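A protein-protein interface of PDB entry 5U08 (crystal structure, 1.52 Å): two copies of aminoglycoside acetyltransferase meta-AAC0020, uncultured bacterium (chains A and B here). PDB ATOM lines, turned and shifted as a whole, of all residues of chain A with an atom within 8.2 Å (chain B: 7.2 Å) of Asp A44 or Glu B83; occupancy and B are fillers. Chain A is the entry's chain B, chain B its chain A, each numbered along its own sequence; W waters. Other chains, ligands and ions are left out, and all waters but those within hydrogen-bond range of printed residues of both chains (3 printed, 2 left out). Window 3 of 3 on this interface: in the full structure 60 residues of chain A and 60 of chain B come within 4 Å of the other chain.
No position is printed for both chains. Of the 14 pairs that touch across the chains among the printed residues, none has its exchanged pair printed and touching as well.
The backbone carbonyl oxygen (O) of Gln B79 is in hydrogen-bond range of a ring nitrogen (NE2) of His A47, 2.8 Å away. A ring nitrogen (NE2) of His A47 sits at hydrogen-bond distance from the backbone carbonyl oxygen (O) of Ser B82. The side-chain carboxylate (OD2) of Asp A44 lies close to the side-chain carboxylate (OE2) of Glu B83, 2.8 Å away.
Of the 12 printed residues of chain B, 6 touch a printed residue of chain A. Hydrophobic or aromatic side chains of chain B within 4 Å of the printed part of chain A: Tyr B80. Among the printed residues, 14 pairs touch across the chains. Among the printed residues, no Asp or Glu carboxylate lies within 4 Å of a Lys or Arg side-chain nitrogen of the other chain.
Water W3 bridges a ring nitrogen (ND1) of His A47 (2.7 Å) and the side-chain carboxylate (OE1) of Glu B83 (3.4 Å). Water W2 bridges OD1 of Asp A44 and OE1 of Glu B83. Water W1 bridges O of Tyr B81 and N of Ser A41.
The side-chain amide nitrogen (NE2) of Gln B79 is in hydrogen-bond range of the backbone carbonyl oxygen (O) of Lys B84, at 2.7 Å. NE2 of Gln B79 sits at hydrogen-bond distance from OE2 of Glu B121. The backbone NH of Lys B84 lies within hydrogen-bond range of the side-chain hydroxyl of Ser B82, at 2.9 Å. The backbone NH of Glu A46 sits close to the side-chain carboxylate of Asp A44 (3.5 Å). OD1 of Asp A44 lies within hydrogen-bond range of N of His A47 (2.8 Å).
Printed residues of chain B within 4 Å of Asp A44: Glu B83 (2.8 Å). Printed residues of chain A within 4 Å of Gln B79: His A47 and Leu A51. Of the printed residues of chain A, Tyr B80 touches Ile A28 (3.8 Å), Pro A43 (3.2 Å), Leu A48 (3.7 Å) and Leu A51 (3.7 Å). Of chain A, only Pro A43 (3.6 Å) and His A47 (3.4 Å) come within 4 Å of Ser B82. Glu B83 touches two residues of chain A. Lys B84 touches none of the printed residues of chain A.
Tyr B80 touches Ile A28 (CB to CD1, 3.8 Å). Tyr B81 touches Ser A41 (O to O, 3.9 Å). Tyr B80 touches Pro A43 (O to CD, 3.2 Å). C of Tyr B81 touches CG of Pro A43, 3.7 Å away. CE1 of His A47 touches OE1 of Glu B78 (3.1 Å). His A47 touches Glu B83. Tyr B80 touches Leu A48 (O to CD2, 3.7 Å). O of Glu B78 touches CD1 of Leu A51, at 3.9 Å. Leu A51 touches Gln B79 (CD2 to O, 3.7 Å). Leu A51 touches Tyr B80.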
ATOM      1  N   LEU A  21     -12.120   1.337  17.094  1.00  0.00           N
ATOM      2  CA  LEU A  21     -12.864   2.082  16.082  1.00  0.00           C
ATOM      3  C   LEU A  21     -13.929   1.236  15.387  1.00  0.00           C
ATOM      4  O   LEU A  21     -15.036   1.751  15.161  1.00  0.00           O
ATOM      5  CB  LEU A  21     -11.907   2.696  15.047  1.00  0.00           C
ATOM      6  CG  LEU A  21     -12.586   3.479  13.903  1.00  0.00           C
ATOM      7  CD1 LEU A  21     -13.424   4.666  14.414  1.00  0.00           C
ATOM      8  CD2 LEU A  21     -11.577   3.937  12.862  1.00  0.00           C
ATOM      9  N   ILE A  25     -17.872   2.595  15.122  1.00  0.00           N
ATOM     10  CA  ILE A  25     -18.656   2.768  13.895  1.00  0.00           C
ATOM     11  C   ILE A  25     -19.947   1.947  13.946  1.00  0.00           C
ATOM     12  O   ILE A  25     -21.019   2.425  13.539  1.00  0.00           O
ATOM     13  CB  ILE A  25     -17.801   2.431  12.657  1.00  0.00           C
ATOM     14  CG1 ILE A  25     -16.801   3.555  12.371  1.00  0.00           C
ATOM     15  CG2 ILE A  25     -18.684   2.235  11.434  1.00  0.00           C
ATOM     16  CD1 ILE A  25     -15.734   3.151  11.373  1.00  0.00           C
ATOM     17  N   ILE A  28     -22.353   3.875  15.985  1.00  0.00           N
ATOM     18  CA  ILE A  28     -22.890   5.029  15.245  1.00  0.00           C
ATOM     19  C   ILE A  28     -23.972   4.580  14.269  1.00  0.00           C
ATOM     20  O   ILE A  28     -24.999   5.261  14.089  1.00  0.00           O
ATOM     21  CB  ILE A  28     -21.746   5.799  14.552  1.00  0.00           C
ATOM     22  CG1 ILE A  28     -20.826   6.440  15.620  1.00  0.00           C
ATOM     23  CG2 ILE A  28     -22.312   6.917  13.605  1.00  0.00           C
ATOM     24  CD1 ILE A  28     -19.464   6.926  15.046  1.00  0.00           C
ATOM     25  N   SER A  41     -24.456  11.322   6.788  1.00  0.00           N
ATOM     26  CA  SER A  41     -23.248  10.776   6.173  1.00  0.00           C
ATOM     27  C   SER A  41     -22.212  10.656   7.279  1.00  0.00           C
ATOM     28  O   SER A  41     -21.905  11.649   7.952  1.00  0.00           O
ATOM     29  CB  SER A  41     -22.712  11.678   5.047  1.00  0.00           C
ATOM     30  OG  SER A  41     -23.682  11.968   4.057  1.00  0.00           O
ATOM     31  N   ILE A  42     -21.704   9.447   7.500  1.00  0.00           N
ATOM     32  CA  ILE A  42     -20.798   9.244   8.636  1.00  0.00           C
ATOM     33  C   ILE A  42     -19.499  10.007   8.391  1.00  0.00           C
ATOM     34  O   ILE A  42     -19.012  10.059   7.240  1.00  0.00           O
ATOM     35  CB  ILE A  42     -20.540   7.745   8.852  1.00  0.00           C
ATOM     36  CG1 ILE A  42     -19.939   7.478  10.242  1.00  0.00           C
ATOM     37  CG2 ILE A  42     -19.608   7.175   7.793  1.00  0.00           C
ATOM     38  CD1 ILE A  42     -19.975   6.013  10.643  1.00  0.00           C
ATOM     39  N   PRO A  43     -18.947  10.672   9.410  1.00  0.00           N
ATOM     40  CA  PRO A  43     -17.617  11.280   9.274  1.00  0.00           C
ATOM     41  C   PRO A  43     -16.553  10.273   8.868  1.00  0.00           C
ATOM     42  O   PRO A  43     -16.675   9.061   9.083  1.00  0.00           O
ATOM     43  CB  PRO A  43     -17.328  11.826  10.679  1.00  0.00           C
ATOM     44  CG  PRO A  43     -18.693  11.970  11.316  1.00  0.00           C
ATOM     45  CD  PRO A  43     -19.548  10.901  10.735  1.00  0.00           C
ATOM     46  N   ASP A  44     -15.466  10.794   8.305  1.00  0.00           N
ATOM     47  CA  ASP A  44     -14.376   9.904   7.939  1.00  0.00           C
ATOM     48  C   ASP A  44     -13.726   9.288   9.185  1.00  0.00           C
ATOM     49  O   ASP A  44     -13.820   9.811  10.305  1.00  0.00           O
ATOM     50  CB  ASP A  44     -13.335  10.624   7.070  1.00  0.00           C
ATOM     51  CG  ASP A  44     -12.712  11.835   7.739  1.00  0.00           C
ATOM     52  OD1 ASP A  44     -12.261  11.738   8.899  1.00  0.00           O
ATOM     53  OD2 ASP A  44     -12.631  12.888   7.072  1.00  0.00           O
ATOM     54  N   SER A  45     -13.065   8.147   8.981  1.00  0.00           N
ATOM     55  CA  SER A  45     -12.550   7.404  10.121  1.00  0.00           C
ATOM     56  C   SER A  45     -11.378   8.091  10.805  1.00  0.00           C
ATOM     57  O   SER A  45     -11.159   7.860  11.999  1.00  0.00           O
ATOM     58  CB  SER A  45     -12.152   5.989   9.691  1.00  0.00           C
ATOM     59  OG  SER A  45     -13.300   5.266   9.288  1.00  0.00           O
ATOM     60  N   GLU A  46     -10.626   8.939  10.102  1.00  0.00           N
ATOM     61  CA  GLU A  46      -9.621   9.761  10.782  1.00  0.00           C
ATOM     62  C   GLU A  46     -10.256  10.621  11.864  1.00  0.00           C
ATOM     63  O   GLU A  46      -9.746  10.694  12.992  1.00  0.00           O
ATOM     64  CB  GLU A  46      -8.889  10.642   9.766  1.00  0.00           C
ATOM     65  CG  GLU A  46      -7.886  11.595  10.373  1.00  0.00           C
ATOM     66  CD  GLU A  46      -7.167  12.445   9.338  1.00  0.00           C
ATOM     67  OE1 GLU A  46      -6.243  13.190   9.734  1.00  0.00           O
ATOM     68  OE2 GLU A  46      -7.515  12.369   8.137  1.00  0.00           O
ATOM     69  N   HIS A  47     -11.394  11.253  11.543  1.00  0.00           N
ATOM     70  CA  HIS A  47     -12.119  12.062  12.512  1.00  0.00           C
ATOM     71  C   HIS A  47     -12.605  11.224  13.691  1.00  0.00           C
ATOM     72  O   HIS A  47     -12.434  11.613  14.857  1.00  0.00           O
ATOM     73  CB  HIS A  47     -13.305  12.755  11.834  1.00  0.00           C
ATOM     74  CG  HIS A  47     -14.127  13.532  12.800  1.00  0.00           C
ATOM     75  ND1 HIS A  47     -13.684  14.718  13.332  1.00  0.00           N
ATOM     76  CD2 HIS A  47     -15.299  13.252  13.413  1.00  0.00           C
ATOM     77  CE1 HIS A  47     -14.567  15.157  14.213  1.00  0.00           C
ATOM     78  NE2 HIS A  47     -15.565  14.297  14.264  1.00  0.00           N
ATOM     79  N   LEU A  48     -13.242  10.082  13.400  1.00  0.00           N
ATOM     80  CA  LEU A  48     -13.792   9.263  14.477  1.00  0.00           C
ATOM     81  C   LEU A  48     -12.685   8.692  15.346  1.00  0.00           C
ATOM     82  O   LEU A  48     -12.856   8.589  16.566  1.00  0.00           O
ATOM     83  CB  LEU A  48     -14.677   8.144  13.921  1.00  0.00           C
ATOM     84  CG  LEU A  48     -15.865   8.700  13.113  1.00  0.00           C
ATOM     85  CD1 LEU A  48     -16.586   7.534  12.501  1.00  0.00           C
ATOM     86  CD2 LEU A  48     -16.801   9.498  14.038  1.00  0.00           C
ATOM     87  N   GLN A  49     -11.537   8.328  14.748  1.00  0.00           N
ATOM     88  CA  GLN A  49     -10.427   7.842  15.578  1.00  0.00           C
ATOM     89  C   GLN A  49      -9.910   8.934  16.505  1.00  0.00           C
ATOM     90  O   GLN A  49      -9.613   8.684  17.683  1.00  0.00           O
ATOM     91  CB  GLN A  49      -9.299   7.304  14.685  1.00  0.00           C
ATOM     92  CG  GLN A  49      -8.136   6.727  15.508  1.00  0.00           C
ATOM     93  CD  GLN A  49      -8.501   5.425  16.209  1.00  0.00           C
ATOM     94  OE1 GLN A  49      -8.741   4.416  15.565  1.00  0.00           O
ATOM     95  NE2 GLN A  49      -8.515   5.441  17.535  1.00  0.00           N
ATOM     96  N   LYS A  50      -9.780  10.155  15.992  1.00  0.00           N
ATOM     97  CA  LYS A  50      -9.331  11.256  16.837  1.00  0.00           C
ATOM     98  C   LYS A  50     -10.267  11.457  18.015  1.00  0.00           C
ATOM     99  O   LYS A  50      -9.812  11.677  19.142  1.00  0.00           O
ATOM    100  CB  LYS A  50      -9.231  12.537  15.998  1.00  0.00           C
ATOM    101  CG  LYS A  50      -8.088  12.511  14.982  1.00  0.00           C
ATOM    102  CD  LYS A  50      -7.605  13.902  14.589  1.00  0.00           C
ATOM    103  CE  LYS A  50      -7.901  14.218  13.124  1.00  0.00           C
ATOM    104  NZ  LYS A  50      -6.723  14.033  12.225  1.00  0.00           N
ATOM    105  N   LEU A  51     -11.582  11.362  17.780  1.00  0.00           N
ATOM    106  CA  LEU A  51     -12.533  11.515  18.883  1.00  0.00           C
ATOM    107  C   LEU A  51     -12.385  10.389  19.896  1.00  0.00           C
ATOM    108  O   LEU A  51     -12.318  10.637  21.113  1.00  0.00           O
ATOM    109  CB  LEU A  51     -13.953  11.583  18.327  1.00  0.00           C
ATOM    110  CG  LEU A  51     -15.115  11.596  19.324  1.00  0.00           C
ATOM    111  CD1 LEU A  51     -14.986  12.736  20.349  1.00  0.00           C
ATOM    112  CD2 LEU A  51     -16.459  11.669  18.563  1.00  0.00           C
ATOM    113  N   GLU B  78     -16.826  17.679  20.564  1.00  0.00           N
ATOM    114  CA  GLU B  78     -16.571  17.082  19.255  1.00  0.00           C
ATOM    115  C   GLU B  78     -17.624  16.017  18.973  1.00  0.00           C
ATOM    116  O   GLU B  78     -17.928  15.186  19.833  1.00  0.00           O
ATOM    117  CB  GLU B  78     -15.170  16.474  19.240  1.00  0.00           C
ATOM    118  CG  GLU B  78     -14.585  16.189  17.864  1.00  0.00           C
ATOM    119  CD  GLU B  78     -14.226  17.484  17.094  1.00  0.00           C
ATOM    120  OE1 GLU B  78     -14.765  17.681  15.986  1.00  0.00           O
ATOM    121  OE2 GLU B  78     -13.414  18.284  17.603  1.00  0.00           O
ATOM    122  N   GLN B  79     -18.164  16.028  17.759  1.00  0.00           N
ATOM    123  CA  GLN B  79     -19.270  15.155  17.386  1.00  0.00           C
ATOM    124  C   GLN B  79     -18.789  13.930  16.628  1.00  0.00           C
ATOM    125  O   GLN B  79     -17.749  13.951  15.956  1.00  0.00           O
ATOM    126  CB  GLN B  79     -20.279  15.891  16.482  1.00  0.00           C
ATOM    127  CG  GLN B  79     -20.874  17.112  17.137  1.00  0.00           C
ATOM    128  CD  GLN B  79     -22.100  17.541  16.384  1.00  0.00           C
ATOM    129  OE1 GLN B  79     -23.176  16.961  16.574  1.00  0.00           O
ATOM    130  NE2 GLN B  79     -21.948  18.520  15.487  1.00  0.00           N
ATOM    131  N   TYR B  80     -19.564  12.850  16.732  1.00  0.00           N
ATOM    132  CA  TYR B  80     -19.362  11.675  15.895  1.00  0.00           C
ATOM    133  C   TYR B  80     -20.356  11.648  14.736  1.00  0.00           C
ATOM    134  O   TYR B  80     -20.249  10.784  13.866  1.00  0.00           O
ATOM    135  CB  TYR B  80     -19.444  10.362  16.727  1.00  0.00           C
ATOM    136  CG  TYR B  80     -20.532  10.403  17.781  1.00  0.00           C
ATOM    137  CD1 TYR B  80     -21.835   9.968  17.472  1.00  0.00           C
ATOM    138  CD2 TYR B  80     -20.269  10.908  19.056  1.00  0.00           C
ATOM    139  CE1 TYR B  80     -22.860  10.052  18.420  1.00  0.00           C
ATOM    140  CE2 TYR B  80     -21.274  10.987  20.017  1.00  0.00           C
ATOM    141  CZ  TYR B  80     -22.554  10.526  19.695  1.00  0.00           C
ATOM    142  OH  TYR B  80     -23.536  10.597  20.643  1.00  0.00           O
ATOM    143  N   TYR B  81     -21.300  12.599  14.678  1.00  0.00           N
ATOM    144  CA  TYR B  81     -22.222  12.670  13.544  1.00  0.00           C
ATOM    145  C   TYR B  81     -21.734  13.630  12.473  1.00  0.00           C
ATOM    146  O   TYR B  81     -22.241  13.594  11.340  1.00  0.00           O
ATOM    147  CB  TYR B  81     -23.619  13.135  13.995  1.00  0.00           C
ATOM    148  CG  TYR B  81     -24.379  12.200  14.933  1.00  0.00           C
ATOM    149  CD1 TYR B  81     -24.428  10.837  14.717  1.00  0.00           C
ATOM    150  CD2 TYR B  81     -25.049  12.725  16.033  1.00  0.00           C
ATOM    151  CE1 TYR B  81     -25.135   9.984  15.597  1.00  0.00           C
ATOM    152  CE2 TYR B  81     -25.772  11.919  16.889  1.00  0.00           C
ATOM    153  CZ  TYR B  81     -25.822  10.554  16.671  1.00  0.00           C
ATOM    154  OH  TYR B  81     -26.517   9.722  17.541  1.00  0.00           O
ATOM    155  N   SER B  82     -20.804  14.511  12.836  1.00  0.00           N
ATOM    156  CA  SER B  82     -20.326  15.583  11.972  1.00  0.00           C
ATOM    157  C   SER B  82     -18.883  15.905  12.337  1.00  0.00           C
ATOM    158  O   SER B  82     -18.490  15.802  13.502  1.00  0.00           O
ATOM    159  CB  SER B  82     -21.180  16.846  12.136  1.00  0.00           C
ATOM    160  OG  SER B  82     -20.646  17.923  11.383  1.00  0.00           O
ATOM    161  N   GLU B  83     -18.120  16.380  11.350  1.00  0.00           N
ATOM    162  CA  GLU B  83     -16.808  16.942  11.644  1.00  0.00           C
ATOM    163  C   GLU B  83     -16.875  18.359  12.190  1.00  0.00           C
ATOM    164  O   GLU B  83     -15.847  18.881  12.630  1.00  0.00           O
ATOM    165  CB  GLU B  83     -15.935  16.933  10.379  1.00  0.00           C
ATOM    166  CG  GLU B  83     -15.269  15.612  10.110  1.00  0.00           C
ATOM    167  CD  GLU B  83     -14.087  15.725   9.157  1.00  0.00           C
ATOM    168  OE1 GLU B  83     -13.145  16.507   9.422  1.00  0.00           O
ATOM    169  OE2 GLU B  83     -14.105  15.019   8.137  1.00  0.00           O
ATOM    170  N   LYS B  84     -18.054  18.997  12.193  1.00  0.00           N
ATOM    171  CA  LYS B  84     -18.201  20.309  12.810  1.00  0.00           C
ATOM    172  C   LYS B  84     -18.648  20.164  14.255  1.00  0.00           C
ATOM    173  O   LYS B  84     -19.703  19.568  14.503  1.00  0.00           O
ATOM    174  CB  LYS B  84     -19.236  21.129  12.056  1.00  0.00           C
ATOM    175  CG  LYS B  84     -19.070  21.118  10.583  1.00  0.00           C
ATOM    176  CD  LYS B  84     -20.153  21.955   9.920  1.00  0.00           C
ATOM    177  CE  LYS B  84     -19.540  22.863   8.874  1.00  0.00           C
ATOM    178  NZ  LYS B  84     -18.863  24.030   9.523  1.00  0.00           N
ATOM    179  N   PRO B  85     -17.907  20.700  15.233  1.00  0.00           N
ATOM    180  CA  PRO B  85     -18.265  20.506  16.644  1.00  0.00           C
ATOM    181  C   PRO B  85     -19.504  21.287  17.078  1.00  0.00           C
ATOM    182  O   PRO B  85     -20.045  22.150  16.378  1.00  0.00           O
ATOM    183  CB  PRO B  85     -17.032  20.987  17.417  1.00  0.00           C
ATOM    184  CG  PRO B  85     -15.923  21.049  16.399  1.00  0.00           C
ATOM    185  CD  PRO B  85     -16.578  21.317  15.077  1.00  0.00           C
ATOM    186  N   LYS B 118     -14.755  29.373  13.934  1.00  0.00           N
ATOM    187  CA  LYS B 118     -14.120  28.072  14.092  1.00  0.00           C
ATOM    188  C   LYS B 118     -14.852  26.955  13.361  1.00  0.00           C
ATOM    189  O   LYS B 118     -14.435  25.792  13.462  1.00  0.00           O
ATOM    190  CB  LYS B 118     -14.008  27.741  15.585  1.00  0.00           C
ATOM    191  CG  LYS B 118     -12.946  28.539  16.286  1.00  0.00           C
ATOM    192  CD  LYS B 118     -13.073  28.360  17.767  1.00  0.00           C
ATOM    193  CE  LYS B 118     -12.722  26.940  18.179  1.00  0.00           C
ATOM    194  NZ  LYS B 118     -11.245  26.725  18.175  1.00  0.00           N
ATOM    195  N   GLY B 119     -15.923  27.256  12.635  1.00  0.00           N
ATOM    196  CA  GLY B 119     -16.566  26.233  11.826  1.00  0.00           C
ATOM    197  C   GLY B 119     -17.431  25.276  12.603  1.00  0.00           C
ATOM    198  O   GLY B 119     -17.647  24.138  12.160  1.00  0.00           O
ATOM    199  N   PHE B 120     -17.943  25.699  13.754  1.00  0.00           N
ATOM    200  CA  PHE B 120     -18.821  24.827  14.514  1.00  0.00           C
ATOM    201  C   PHE B 120     -20.194  24.743  13.854  1.00  0.00           C
ATOM    202  O   PHE B 120     -20.608  25.628  13.078  1.00  0.00           O
ATOM    203  CB  PHE B 120     -18.981  25.353  15.948  1.00  0.00           C
ATOM    204  CG  PHE B 120     -17.854  24.982  16.882  1.00  0.00           C
ATOM    205  CD1 PHE B 120     -16.527  25.022  16.469  1.00  0.00           C
ATOM    206  CD2 PHE B 120     -18.137  24.601  18.196  1.00  0.00           C
ATOM    207  CE1 PHE B 120     -15.499  24.669  17.342  1.00  0.00           C
ATOM    208  CE2 PHE B 120     -17.119  24.257  19.088  1.00  0.00           C
ATOM    209  CZ  PHE B 120     -15.805  24.276  18.667  1.00  0.00           C
ATOM    210  N   GLU B 121     -20.930  23.688  14.199  1.00  0.00           N
ATOM    211  CA  GLU B 121     -22.269  23.507  13.637  1.00  0.00           C
ATOM    212  C   GLU B 121     -23.318  24.289  14.419  1.00  0.00           C
ATOM    213  O   GLU B 121     -24.238  24.879  13.829  1.00  0.00           O
ATOM    214  CB  GLU B 121     -22.637  22.005  13.623  1.00  0.00           C
ATOM    215  CG  GLU B 121     -24.029  21.758  13.084  1.00  0.00           C
ATOM    216  CD  GLU B 121     -24.497  20.336  13.280  1.00  0.00           C
ATOM    217  OE1 GLU B 121     -25.708  20.111  13.135  1.00  0.00           O
ATOM    218  OE2 GLU B 121     -23.664  19.447  13.559  1.00  0.00           O
HETATM  219  O   HOH W   1     -24.356  13.661   9.032  1.00  0.00           O
HETATM  220  O   HOH W   2     -10.787  14.045   9.136  1.00  0.00           O
HETATM  221  O   HOH W   3     -11.515  16.090  12.385  1.00  0.00           O
